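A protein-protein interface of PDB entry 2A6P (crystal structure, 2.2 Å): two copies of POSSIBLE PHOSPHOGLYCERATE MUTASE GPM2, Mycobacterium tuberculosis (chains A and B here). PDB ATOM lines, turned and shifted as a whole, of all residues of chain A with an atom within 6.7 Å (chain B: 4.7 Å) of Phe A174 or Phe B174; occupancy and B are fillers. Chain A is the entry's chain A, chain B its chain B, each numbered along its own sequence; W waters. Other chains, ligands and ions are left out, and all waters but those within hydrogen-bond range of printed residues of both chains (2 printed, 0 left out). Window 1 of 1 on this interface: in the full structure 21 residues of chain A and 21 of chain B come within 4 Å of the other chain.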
ATOM      1  N   TRP A 114     -10.989 -15.331  30.121  1.00  0.00           N
ATOM      2  CA  TRP A 114     -12.167 -14.845  30.845  1.00  0.00           C
ATOM      3  C   TRP A 114     -12.405 -15.403  32.240  1.00  0.00           C
ATOM      4  O   TRP A 114     -13.000 -14.731  33.091  1.00  0.00           O
ATOM      5  CB  TRP A 114     -13.421 -15.092  30.001  1.00  0.00           C
ATOM      6  CG  TRP A 114     -13.250 -14.552  28.650  1.00  0.00           C
ATOM      7  CD1 TRP A 114     -12.950 -15.248  27.513  1.00  0.00           C
ATOM      8  CD2 TRP A 114     -13.244 -13.168  28.296  1.00  0.00           C
ATOM      9  NE1 TRP A 114     -12.749 -14.373  26.468  1.00  0.00           N
ATOM     10  CE2 TRP A 114     -12.923 -13.090  26.923  1.00  0.00           C
ATOM     11  CE3 TRP A 114     -13.478 -11.982  29.009  1.00  0.00           C
ATOM     12  CZ2 TRP A 114     -12.822 -11.866  26.246  1.00  0.00           C
ATOM     13  CZ3 TRP A 114     -13.381 -10.766  28.336  1.00  0.00           C
ATOM     14  CH2 TRP A 114     -13.054 -10.719  26.967  1.00  0.00           C
ATOM     15  N   GLY A 153      -9.022  -6.890  20.963  1.00  0.00           N
ATOM     16  CA  GLY A 153     -10.013  -7.953  21.000  1.00  0.00           C
ATOM     17  C   GLY A 153     -10.637  -8.257  22.340  1.00  0.00           C
ATOM     18  O   GLY A 153     -11.848  -8.056  22.539  1.00  0.00           O
ATOM     19  N   ARG A 157     -14.159  -6.626  24.159  1.00  0.00           N
ATOM     20  CA  ARG A 157     -15.189  -7.555  24.597  1.00  0.00           C
ATOM     21  C   ARG A 157     -15.487  -7.342  26.069  1.00  0.00           C
ATOM     22  O   ARG A 157     -16.620  -7.531  26.514  1.00  0.00           O
ATOM     23  CB  ARG A 157     -14.731  -8.993  24.451  1.00  0.00           C
ATOM     24  CG  ARG A 157     -14.518  -9.516  23.062  1.00  0.00           C
ATOM     25  CD  ARG A 157     -14.380 -11.012  23.249  1.00  0.00           C
ATOM     26  NE  ARG A 157     -13.581 -11.652  22.234  1.00  0.00           N
ATOM     27  CZ  ARG A 157     -13.387 -12.961  22.181  1.00  0.00           C
ATOM     28  NH1 ARG A 157     -13.952 -13.747  23.091  1.00  0.00           N
ATOM     29  NH2 ARG A 157     -12.618 -13.469  21.231  1.00  0.00           N
ATOM     30  N   ILE A 160     -17.692  -4.357  26.315  1.00  0.00           N
ATOM     31  CA  ILE A 160     -19.042  -4.738  25.879  1.00  0.00           C
ATOM     32  C   ILE A 160     -19.758  -5.567  26.941  1.00  0.00           C
ATOM     33  O   ILE A 160     -20.921  -5.302  27.265  1.00  0.00           O
ATOM     34  CB  ILE A 160     -18.989  -5.547  24.567  1.00  0.00           C
ATOM     35  CG1 ILE A 160     -18.497  -4.649  23.427  1.00  0.00           C
ATOM     36  CG2 ILE A 160     -20.354  -6.140  24.257  1.00  0.00           C
ATOM     37  CD1 ILE A 160     -18.250  -5.393  22.154  1.00  0.00           C
ATOM     38  N   THR A 161     -19.063  -6.576  27.469  1.00  0.00           N
ATOM     39  CA  THR A 161     -19.637  -7.441  28.496  1.00  0.00           C
ATOM     40  C   THR A 161     -20.092  -6.628  29.701  1.00  0.00           C
ATOM     41  O   THR A 161     -21.128  -6.911  30.290  1.00  0.00           O
ATOM     42  CB  THR A 161     -18.622  -8.497  28.972  1.00  0.00           C
ATOM     43  OG1 THR A 161     -18.223  -9.309  27.862  1.00  0.00           O
ATOM     44  CG2 THR A 161     -19.233  -9.390  30.033  1.00  0.00           C
ATOM     45  N   VAL A 164     -23.215  -4.287  29.076  1.00  0.00           N
ATOM     46  CA  VAL A 164     -24.450  -5.038  29.241  1.00  0.00           C
ATOM     47  C   VAL A 164     -24.616  -5.640  30.638  1.00  0.00           C
ATOM     48  O   VAL A 164     -25.479  -6.481  30.860  1.00  0.00           O
ATOM     49  CB  VAL A 164     -24.572  -6.149  28.170  1.00  0.00           C
ATOM     50  CG1 VAL A 164     -24.682  -5.514  26.796  1.00  0.00           C
ATOM     51  CG2 VAL A 164     -23.382  -7.081  28.227  1.00  0.00           C
ATOM     52  N   LEU A 166     -22.882  -7.804  32.624  1.00  0.00           N
ATOM     53  CA  LEU A 166     -22.723  -9.235  32.840  1.00  0.00           C
ATOM     54  C   LEU A 166     -21.353  -9.466  33.498  1.00  0.00           C
ATOM     55  O   LEU A 166     -20.491  -8.584  33.460  1.00  0.00           O
ATOM     56  CB  LEU A 166     -22.774  -9.980  31.497  1.00  0.00           C
ATOM     57  CG  LEU A 166     -24.100 -10.043  30.733  1.00  0.00           C
ATOM     58  CD1 LEU A 166     -23.850 -10.525  29.313  1.00  0.00           C
ATOM     59  CD2 LEU A 166     -25.070 -10.975  31.454  1.00  0.00           C
ATOM     60  N   GLU A 170     -18.334 -13.722  30.897  1.00  0.00           N
ATOM     61  CA  GLU A 170     -19.133 -13.807  29.674  1.00  0.00           C
ATOM     62  C   GLU A 170     -18.460 -13.214  28.426  1.00  0.00           C
ATOM     63  O   GLU A 170     -19.028 -13.275  27.331  1.00  0.00           O
ATOM     64  CB  GLU A 170     -20.502 -13.126  29.876  1.00  0.00           C
ATOM     65  CG  GLU A 170     -21.361 -13.650  31.025  1.00  0.00           C
ATOM     66  CD  GLU A 170     -21.606 -15.152  30.968  1.00  0.00           C
ATOM     67  OE1 GLU A 170     -21.505 -15.754  29.881  1.00  0.00           O
ATOM     68  OE2 GLU A 170     -21.925 -15.738  32.019  1.00  0.00           O
ATOM     69  N   GLY A 171     -17.266 -12.638  28.584  1.00  0.00           N
ATOM     70  CA  GLY A 171     -16.576 -12.077  27.434  1.00  0.00           C
ATOM     71  C   GLY A 171     -16.298 -13.127  26.359  1.00  0.00           C
ATOM     72  O   GLY A 171     -16.031 -12.803  25.197  1.00  0.00           O
ATOM     73  N   SER A 172     -16.364 -14.396  26.755  1.00  0.00           N
ATOM     74  CA  SER A 172     -16.125 -15.524  25.859  1.00  0.00           C
ATOM     75  C   SER A 172     -17.266 -15.704  24.861  1.00  0.00           C
ATOM     76  O   SER A 172     -17.101 -16.346  23.831  1.00  0.00           O
ATOM     77  CB  SER A 172     -15.979 -16.811  26.681  1.00  0.00           C
ATOM     78  OG  SER A 172     -17.184 -17.109  27.395  1.00  0.00           O
ATOM     79  N   ARG A 173     -18.420 -15.123  25.179  1.00  0.00           N
ATOM     80  CA  ARG A 173     -19.621 -15.232  24.348  1.00  0.00           C
ATOM     81  C   ARG A 173     -19.753 -14.207  23.221  1.00  0.00           C
ATOM     82  O   ARG A 173     -20.746 -14.227  22.489  1.00  0.00           O
ATOM     83  CB  ARG A 173     -20.856 -15.146  25.242  1.00  0.00           C
ATOM     84  CG  ARG A 173     -20.822 -16.098  26.426  1.00  0.00           C
ATOM     85  CD  ARG A 173     -20.766 -17.551  25.957  1.00  0.00           C
ATOM     86  NE  ARG A 173     -20.852 -18.496  27.073  1.00  0.00           N
ATOM     87  CZ  ARG A 173     -21.166 -19.780  26.936  1.00  0.00           C
ATOM     88  NH1 ARG A 173     -21.422 -20.269  25.727  1.00  0.00           N
ATOM     89  NH2 ARG A 173     -21.236 -20.571  28.001  1.00  0.00           N
ATOM     90  N   PHE A 174     -18.767 -13.325  23.071  1.00  0.00           N
ATOM     91  CA  PHE A 174     -18.823 -12.303  22.037  1.00  0.00           C
ATOM     92  C   PHE A 174     -17.562 -12.252  21.187  1.00  0.00           C
ATOM     93  O   PHE A 174     -16.464 -12.109  21.719  1.00  0.00           O
ATOM     94  CB  PHE A 174     -19.034 -10.921  22.663  1.00  0.00           C
ATOM     95  CG  PHE A 174     -20.160 -10.868  23.658  1.00  0.00           C
ATOM     96  CD1 PHE A 174     -19.897 -10.818  25.031  1.00  0.00           C
ATOM     97  CD2 PHE A 174     -21.480 -10.888  23.228  1.00  0.00           C
ATOM     98  CE1 PHE A 174     -20.932 -10.788  25.967  1.00  0.00           C
ATOM     99  CE2 PHE A 174     -22.535 -10.860  24.154  1.00  0.00           C
ATOM    100  CZ  PHE A 174     -22.258 -10.811  25.533  1.00  0.00           C
ATOM    101  N   ALA A 175     -17.719 -12.353  19.871  1.00  0.00           N
ATOM    102  CA  ALA A 175     -16.569 -12.295  18.970  1.00  0.00           C
ATOM    103  C   ALA A 175     -16.177 -10.833  18.759  1.00  0.00           C
ATOM    104  O   ALA A 175     -16.964  -9.921  19.036  1.00  0.00           O
ATOM    105  CB  ALA A 175     -16.906 -12.935  17.635  1.00  0.00           C
ATOM    106  N   MET A 176     -14.962 -10.619  18.264  1.00  0.00           N
ATOM    107  CA  MET A 176     -14.440  -9.285  17.999  1.00  0.00           C
ATOM    108  C   MET A 176     -13.242  -9.480  17.089  1.00  0.00           C
ATOM    109  O   MET A 176     -12.101  -9.445  17.549  1.00  0.00           O
ATOM    110  CB  MET A 176     -13.979  -8.610  19.297  1.00  0.00           C
ATOM    111  CG  MET A 176     -13.737  -7.090  19.204  1.00  0.00           C
ATOM    112  SD  MET A 176     -15.259  -6.045  19.300  1.00  0.00           S
ATOM    113  CE  MET A 176     -14.718  -4.589  18.405  1.00  0.00           C
ATOM    114  N   GLU A 187     -32.140   0.429  24.979  1.00  0.00           N
ATOM    115  CA  GLU A 187     -33.461   0.078  24.467  1.00  0.00           C
ATOM    116  C   GLU A 187     -34.381   0.128  25.688  1.00  0.00           C
ATOM    117  O   GLU A 187     -34.182  -0.623  26.650  1.00  0.00           O
ATOM    118  CB  GLU A 187     -33.495  -1.332  23.861  1.00  0.00           C
ATOM    119  CG  GLU A 187     -34.539  -1.461  22.742  1.00  0.00           C
ATOM    120  CD  GLU A 187     -35.186  -2.846  22.635  1.00  0.00           C
ATOM    121  OE1 GLU A 187     -34.488  -3.871  22.809  1.00  0.00           O
ATOM    122  OE2 GLU A 187     -36.408  -2.900  22.351  1.00  0.00           O
ATOM    123  N   ARG A 191     -29.199  -0.747  29.031  1.00  0.00           N
ATOM    124  CA  ARG A 191     -27.935  -0.704  28.300  1.00  0.00           C
ATOM    125  C   ARG A 191     -27.930  -1.978  27.456  1.00  0.00           C
ATOM    126  O   ARG A 191     -28.150  -3.080  27.963  1.00  0.00           O
ATOM    127  CB  ARG A 191     -26.751  -0.654  29.277  1.00  0.00           C
ATOM    128  CG  ARG A 191     -26.164   0.746  29.404  1.00  0.00           C
ATOM    129  CD  ARG A 191     -25.538   1.031  30.757  1.00  0.00           C
ATOM    130  NE  ARG A 191     -24.556   0.030  31.167  1.00  0.00           N
ATOM    131  CZ  ARG A 191     -23.782   0.159  32.243  1.00  0.00           C
ATOM    132  NH1 ARG A 191     -23.879   1.250  33.002  1.00  0.00           N
ATOM    133  NH2 ARG A 191     -22.926  -0.801  32.570  1.00  0.00           N
ATOM    134  N   GLN A 192     -27.683  -1.824  26.163  1.00  0.00           N
ATOM    135  CA  GLN A 192     -27.750  -2.961  25.255  1.00  0.00           C
ATOM    136  C   GLN A 192     -26.678  -2.979  24.169  1.00  0.00           C
ATOM    137  O   GLN A 192     -26.136  -1.936  23.807  1.00  0.00           O
ATOM    138  CB  GLN A 192     -29.171  -2.959  24.631  1.00  0.00           C
ATOM    139  CG  GLN A 192     -29.356  -3.584  23.239  1.00  0.00           C
ATOM    140  CD  GLN A 192     -30.798  -3.433  22.730  1.00  0.00           C
ATOM    141  OE1 GLN A 192     -31.721  -4.107  23.207  1.00  0.00           O
ATOM    142  NE2 GLN A 192     -30.996  -2.538  21.775  1.00  0.00           N
ATOM    143  N   LEU A 193     -26.370  -4.181  23.679  1.00  0.00           N
ATOM    144  CA  LEU A 193     -25.407  -4.380  22.585  1.00  0.00           C
ATOM    145  C   LEU A 193     -26.256  -4.267  21.310  1.00  0.00           C
ATOM    146  O   LEU A 193     -27.164  -5.085  21.092  1.00  0.00           O
ATOM    147  CB  LEU A 193     -24.789  -5.793  22.638  1.00  0.00           C
ATOM    148  CG  LEU A 193     -23.380  -6.081  22.084  1.00  0.00           C
ATOM    149  CD1 LEU A 193     -23.367  -7.471  21.473  1.00  0.00           C
ATOM    150  CD2 LEU A 193     -22.946  -5.053  21.052  1.00  0.00           C
ATOM    151  N   ALA A 194     -25.963  -3.275  20.474  1.00  0.00           N
ATOM    152  CA  ALA A 194     -26.730  -3.074  19.240  1.00  0.00           C
ATOM    153  C   ALA A 194     -26.127  -3.739  17.994  1.00  0.00           C
ATOM    154  O   ALA A 194     -26.853  -4.356  17.200  1.00  0.00           O
ATOM    155  CB  ALA A 194     -26.923  -1.565  18.989  1.00  0.00           C
ATOM    156  N   LEU A 196     -22.516  -6.003  16.452  1.00  0.00           N
ATOM    157  CA  LEU A 196     -21.319  -6.781  16.750  1.00  0.00           C
ATOM    158  C   LEU A 196     -20.774  -7.420  15.478  1.00  0.00           C
ATOM    159  O   LEU A 196     -21.530  -7.794  14.579  1.00  0.00           O
ATOM    160  CB  LEU A 196     -21.618  -7.887  17.775  1.00  0.00           C
ATOM    161  CG  LEU A 196     -20.389  -8.679  18.263  1.00  0.00           C
ATOM    162  CD1 LEU A 196     -19.458  -7.753  19.033  1.00  0.00           C
ATOM    163  CD2 LEU A 196     -20.808  -9.848  19.147  1.00  0.00           C
ATOM    164  N   ARG B 157     -33.831 -13.136  19.596  1.00  0.00           N
ATOM    165  CA  ARG B 157     -32.984 -12.750  20.720  1.00  0.00           C
ATOM    166  C   ARG B 157     -32.983 -13.848  21.758  1.00  0.00           C
ATOM    167  O   ARG B 157     -31.997 -14.052  22.456  1.00  0.00           O
ATOM    168  CB  ARG B 157     -33.497 -11.493  21.403  1.00  0.00           C
ATOM    169  CG  ARG B 157     -33.454 -10.208  20.615  1.00  0.00           C
ATOM    170  CD  ARG B 157     -33.734  -9.145  21.652  1.00  0.00           C
ATOM    171  NE  ARG B 157     -34.356  -7.955  21.112  1.00  0.00           N
ATOM    172  CZ  ARG B 157     -34.632  -6.880  21.843  1.00  0.00           C
ATOM    173  NH1 ARG B 157     -34.330  -6.853  23.139  1.00  0.00           N
ATOM    174  NH2 ARG B 157     -35.233  -5.846  21.275  1.00  0.00           N
ATOM    175  N   THR B 161     -29.672 -15.571  23.074  1.00  0.00           N
ATOM    176  CA  THR B 161     -29.385 -15.557  24.505  1.00  0.00           C
ATOM    177  C   THR B 161     -29.140 -16.976  25.005  1.00  0.00           C
ATOM    178  O   THR B 161     -28.289 -17.210  25.857  1.00  0.00           O
ATOM    179  CB  THR B 161     -30.562 -14.942  25.297  1.00  0.00           C
ATOM    180  OG1 THR B 161     -30.783 -13.595  24.858  1.00  0.00           O
ATOM    181  CG2 THR B 161     -30.273 -14.951  26.786  1.00  0.00           C
ATOM    182  N   LEU B 166     -27.072 -18.038  28.529  1.00  0.00           N
ATOM    183  CA  LEU B 166     -27.377 -17.042  29.554  1.00  0.00           C
ATOM    184  C   LEU B 166     -28.859 -17.187  29.911  1.00  0.00           C
ATOM    185  O   LEU B 166     -29.613 -17.815  29.166  1.00  0.00           O
ATOM    186  CB  LEU B 166     -27.126 -15.626  29.016  1.00  0.00           C
ATOM    187  CG  LEU B 166     -25.686 -15.205  28.717  1.00  0.00           C
ATOM    188  CD1 LEU B 166     -25.704 -13.909  27.916  1.00  0.00           C
ATOM    189  CD2 LEU B 166     -24.904 -15.031  30.021  1.00  0.00           C
ATOM    190  N   GLU B 170     -31.608 -12.051  29.950  1.00  0.00           N
ATOM    191  CA  GLU B 170     -30.595 -11.272  29.236  1.00  0.00           C
ATOM    192  C   GLU B 170     -30.959 -10.921  27.786  1.00  0.00           C
ATOM    193  O   GLU B 170     -30.187 -10.232  27.100  1.00  0.00           O
ATOM    194  CB  GLU B 170     -29.249 -12.012  29.246  1.00  0.00           C
ATOM    195  CG  GLU B 170     -28.688 -12.377  30.625  1.00  0.00           C
ATOM    196  CD  GLU B 170     -28.545 -11.192  31.571  1.00  0.00           C
ATOM    197  OE1 GLU B 170     -28.481 -10.033  31.114  1.00  0.00           O
ATOM    198  OE2 GLU B 170     -28.476 -11.427  32.794  1.00  0.00           O
ATOM    199  N   GLY B 171     -32.118 -11.390  27.317  1.00  0.00           N
ATOM    200  CA  GLY B 171     -32.535 -11.077  25.960  1.00  0.00           C
ATOM    201  C   GLY B 171     -32.654  -9.579  25.757  1.00  0.00           C
ATOM    202  O   GLY B 171     -32.607  -9.086  24.630  1.00  0.00           O
ATOM    203  N   SER B 172     -32.810  -8.846  26.857  1.00  0.00           N
ATOM    204  CA  SER B 172     -32.923  -7.388  26.812  1.00  0.00           C
ATOM    205  C   SER B 172     -31.624  -6.691  26.388  1.00  0.00           C
ATOM    206  O   SER B 172     -31.638  -5.526  25.971  1.00  0.00           O
ATOM    207  CB  SER B 172     -33.322  -6.853  28.194  1.00  0.00           C
ATOM    208  OG  SER B 172     -32.317  -7.116  29.156  1.00  0.00           O
ATOM    209  N   ARG B 173     -30.511  -7.415  26.492  1.00  0.00           N
ATOM    210  CA  ARG B 173     -29.188  -6.868  26.186  1.00  0.00           C
ATOM    211  C   ARG B 173     -28.759  -6.964  24.725  1.00  0.00           C
ATOM    212  O   ARG B 173     -27.646  -6.552  24.383  1.00  0.00           O
ATOM    213  CB  ARG B 173     -28.133  -7.576  27.055  1.00  0.00           C
ATOM    214  CG  ARG B 173     -28.437  -7.578  28.554  1.00  0.00           C
ATOM    215  CD  ARG B 173     -28.500  -6.154  29.079  1.00  0.00           C
ATOM    216  NE  ARG B 173     -28.753  -6.105  30.516  1.00  0.00           N
ATOM    217  CZ  ARG B 173     -28.524  -5.038  31.271  1.00  0.00           C
ATOM    218  NH1 ARG B 173     -28.033  -3.933  30.727  1.00  0.00           N
ATOM    219  NH2 ARG B 173     -28.784  -5.070  32.570  1.00  0.00           N
ATOM    220  N   PHE B 174     -29.622  -7.518  23.873  1.00  0.00           N
ATOM    221  CA  PHE B 174     -29.295  -7.677  22.459  1.00  0.00           C
ATOM    222  C   PHE B 174     -30.356  -7.094  21.530  1.00  0.00           C
ATOM    223  O   PHE B 174     -31.531  -7.457  21.615  1.00  0.00           O
ATOM    224  CB  PHE B 174     -29.099  -9.166  22.119  1.00  0.00           C
ATOM    225  CG  PHE B 174     -28.182  -9.892  23.068  1.00  0.00           C
ATOM    226  CD1 PHE B 174     -28.698 -10.772  24.018  1.00  0.00           C
ATOM    227  CD2 PHE B 174     -26.808  -9.671  23.037  1.00  0.00           C
ATOM    228  CE1 PHE B 174     -27.866 -11.422  24.930  1.00  0.00           C
ATOM    229  CE2 PHE B 174     -25.962 -10.313  23.943  1.00  0.00           C
ATOM    230  CZ  PHE B 174     -26.492 -11.193  24.893  1.00  0.00           C
ATOM    231  N   ALA B 175     -29.941  -6.198  20.636  1.00  0.00           N
ATOM    232  CA  ALA B 175     -30.881  -5.615  19.683  1.00  0.00           C
ATOM    233  C   ALA B 175     -31.104  -6.616  18.548  1.00  0.00           C
ATOM    234  O   ALA B 175     -30.347  -7.584  18.396  1.00  0.00           O
ATOM    235  CB  ALA B 175     -30.348  -4.309  19.130  1.00  0.00           C
ATOM    236  N   MET B 176     -32.161  -6.380  17.770  1.00  0.00           N
ATOM    237  CA  MET B 176     -32.521  -7.223  16.639  1.00  0.00           C
ATOM    238  C   MET B 176     -33.543  -6.427  15.819  1.00  0.00           C
ATOM    239  O   MET B 176     -34.749  -6.664  15.920  1.00  0.00           O
ATOM    240  CB  MET B 176     -33.144  -8.544  17.128  1.00  0.00           C
ATOM    241  CG  MET B 176     -33.265  -9.667  16.072  1.00  0.00           C
ATOM    242  SD  MET B 176     -31.743 -10.671  15.791  1.00  0.00           S
ATOM    243  CE  MET B 176     -31.974 -11.119  14.082  1.00  0.00           C
ATOM    244  N   GLN B 192     -20.599 -19.012  20.871  1.00  0.00           N
ATOM    245  CA  GLN B 192     -20.460 -17.557  20.893  1.00  0.00           C
ATOM    246  C   GLN B 192     -21.308 -16.783  19.874  1.00  0.00           C
ATOM    247  O   GLN B 192     -21.708 -17.332  18.849  1.00  0.00           O
ATOM    248  CB  GLN B 192     -18.953 -17.244  20.714  1.00  0.00           C
ATOM    249  CG  GLN B 192     -18.574 -15.900  20.118  1.00  0.00           C
ATOM    250  CD  GLN B 192     -17.067 -15.780  19.925  1.00  0.00           C
ATOM    251  OE1 GLN B 192     -16.319 -15.620  20.895  1.00  0.00           O
ATOM    252  NE2 GLN B 192     -16.612 -15.877  18.676  1.00  0.00           N
ATOM    253  N   LEU B 193     -21.586 -15.513  20.187  1.00  0.00           N
ATOM    254  CA  LEU B 193     -22.338 -14.627  19.291  1.00  0.00           C
ATOM    255  C   LEU B 193     -21.260 -13.973  18.419  1.00  0.00           C
ATOM    256  O   LEU B 193     -20.420 -13.242  18.930  1.00  0.00           O
ATOM    257  CB  LEU B 193     -23.079 -13.525  20.083  1.00  0.00           C
ATOM    258  CG  LEU B 193     -24.380 -12.877  19.555  1.00  0.00           C
ATOM    259  CD1 LEU B 193     -24.371 -11.423  19.920  1.00  0.00           C
ATOM    260  CD2 LEU B 193     -24.549 -13.031  18.060  1.00  0.00           C
ATOM    261  N   LEU B 196     -24.067  -9.382  15.060  1.00  0.00           N
ATOM    262  CA  LEU B 196     -25.355  -8.883  15.538  1.00  0.00           C
ATOM    263  C   LEU B 196     -25.668  -7.561  14.853  1.00  0.00           C
ATOM    264  O   LEU B 196     -24.763  -6.786  14.546  1.00  0.00           O
ATOM    265  CB  LEU B 196     -25.347  -8.670  17.065  1.00  0.00           C
ATOM    266  CG  LEU B 196     -26.707  -8.274  17.662  1.00  0.00           C
ATOM    267  CD1 LEU B 196     -27.680  -9.425  17.495  1.00  0.00           C
ATOM    268  CD2 LEU B 196     -26.573  -7.918  19.143  1.00  0.00           C
HETATM  269  O   HOH W   1     -26.843  -8.197  32.697  1.00  0.00           O
HETATM  270  O   HOH W   2     -34.214  -3.737  26.153  1.00  0.00           O
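Ser A172 touches Gln B192, and with the chains exchanged Gln A192 touches Ser B172. Phe B174 touches its own counterpart, Phe A174. Ala A175 touches Gln B192, and with the chains exchanged Gln A192 touches Ala B175. Leu A193 touches Leu B196, and with the chains exchanged Leu A196 touches Leu B193. Positions printed for both chains: 157, 161, 166, 170, 171, 172, 173, 174, 175, 176, 192, 193 and 196.
Of the 13 printed residues of chain B, 10 touch a printed residue of chain A. Hydrophobic or aromatic side chains of chain B within 4 Å of the printed part of chain A: Leu B166, Phe B174, Ala B175, Leu B193 and Leu B196. Of the 20 printed residues of chain A, 14 touch a printed residue of chain B. Printed residues of chain A that touch a printed residue of chain B: Arg A157, Val A164, Leu A166, Glu A170, Ser A172, Arg A173, Phe A174, Ala A175, Glu A187, Arg A191, Gln A192, Leu A193, Ala A194 and Leu A196. Hydrophobic or aromatic side chains of chain A that line the printed part of chain B: Val A164, Leu A166, Phe A174, Ala A175, Leu A193 and Leu A196. Along chain A the printed residues that touch a printed residue of chain B span positions 157 to 196. Among the printed residues, Asp or Glu carboxylates within 4 Å of a Lys or Arg side-chain nitrogen of the other chain: Glu A187 with Arg B157.
O of Thr B161 lies within hydrogen-bond range of N of Leu B166 (3.1 Å). The backbone carbonyl oxygen (O) of Thr A161 sits at hydrogen-bond distance from the backbone NH (N) of Leu A166 (3.1 Å). OE1 of Glu B170 lies within salt-bridge range of NE of Arg B173. The guanidinium group (NH1) of Arg B157 lies close to the backbone carbonyl oxygen (O) of Gly B171. The side-chain carboxylate (OE1) of Glu A170 lies within salt-bridge range of the guanidinium group (NE) of Arg A173, 3.98 Å away. NH1 of Arg A157 is in hydrogen-bond range of O of Gly A171 (3.1 Å).
Water W1 bridges the backbone carbonyl oxygen (O) of Val A164 (2.9 Å) and the side-chain carboxylate (OE1) of Glu B170 (2.9 Å). Water W2 bridges the backbone carbonyl oxygen (O) of Ser B172 (3.1 Å) and the backbone carbonyl oxygen (O) of Glu A187 (3.2 Å).
Gln B192 touches Arg A157. Glu B170 touches Leu A166 (CD to CD2, 3.5 Å). CD of Glu A170 touches CD2 of Leu B166, 3.4 Å away. Arg A173 touches Gln B192. Gln B192 touches Phe A174. Gln A192 touches Arg B173 (CG to O, 3.6 Å). OE1 of Gln A192 touches C of Phe B174, 3.7 Å away. CA of Phe B174 touches O of Leu A193 (3.6 Å). Leu B196 touches Leu A193. Ala B175 touches Ala A194 (CB to CA, 3.8 Å).
Phe A174 touches three residues of chain B. Of the printed residues of chain B, Gln A192 touches Arg B157 (3.8 Å), Ser B172 (3.1 Å), Arg B173 (3.6 Å), Phe B174 (3.7 Å) and Ala B175 (3.2 Å). Of the printed residues of chain A, Ser B172 touches Gln A192. Printed residues of chain A within 4 Å of Leu B193: Arg A173 (2.8 Å), Phe A174 (3.6 Å), Ala A175 (3.0 Å) and Leu A196 (3.4 Å). The nearest printed residue of chain B that does not touch Phe A174 is Leu B166 (5.2 Å). The nearest printed residue of chain B that does not touch Arg A157 is Leu B193 (7.7 Å).
The backbone NH (N) of Leu B193 is in hydrogen-bond range of the backbone carbonyl oxygen (O) of Arg A173. N of Leu A193 is in hydrogen-bond range of O of Arg B173 (2.8 Å). The side-chain carboxylate of Glu A187 lies within salt-bridge range of the guanidinium group of Arg B157, 2.6 Å away. O of Ser A172 lies close to OE1 of Gln B192 (3.1 Å). The backbone carbonyl oxygen (O) of Leu B193 is in hydrogen-bond range of the backbone NH (N) of Ala A175 (3.0 Å). OE1 of Gln A192 lies close to O of Ser B172 (3.1 Å). NE of Arg B173 sits at hydrogen-bond distance from O of Val A164. The backbone carbonyl oxygen of Arg A191 is in hydrogen-bond range of the guanidinium group of Arg B173, at 2.9 Å. The backbone carbonyl oxygen of Leu A196 is in hydrogen-bond range of the backbone NH of Leu B196 (3.0 Å). N of Ala B175 is in hydrogen-bond range of O of Leu A193 (3.0 Å).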
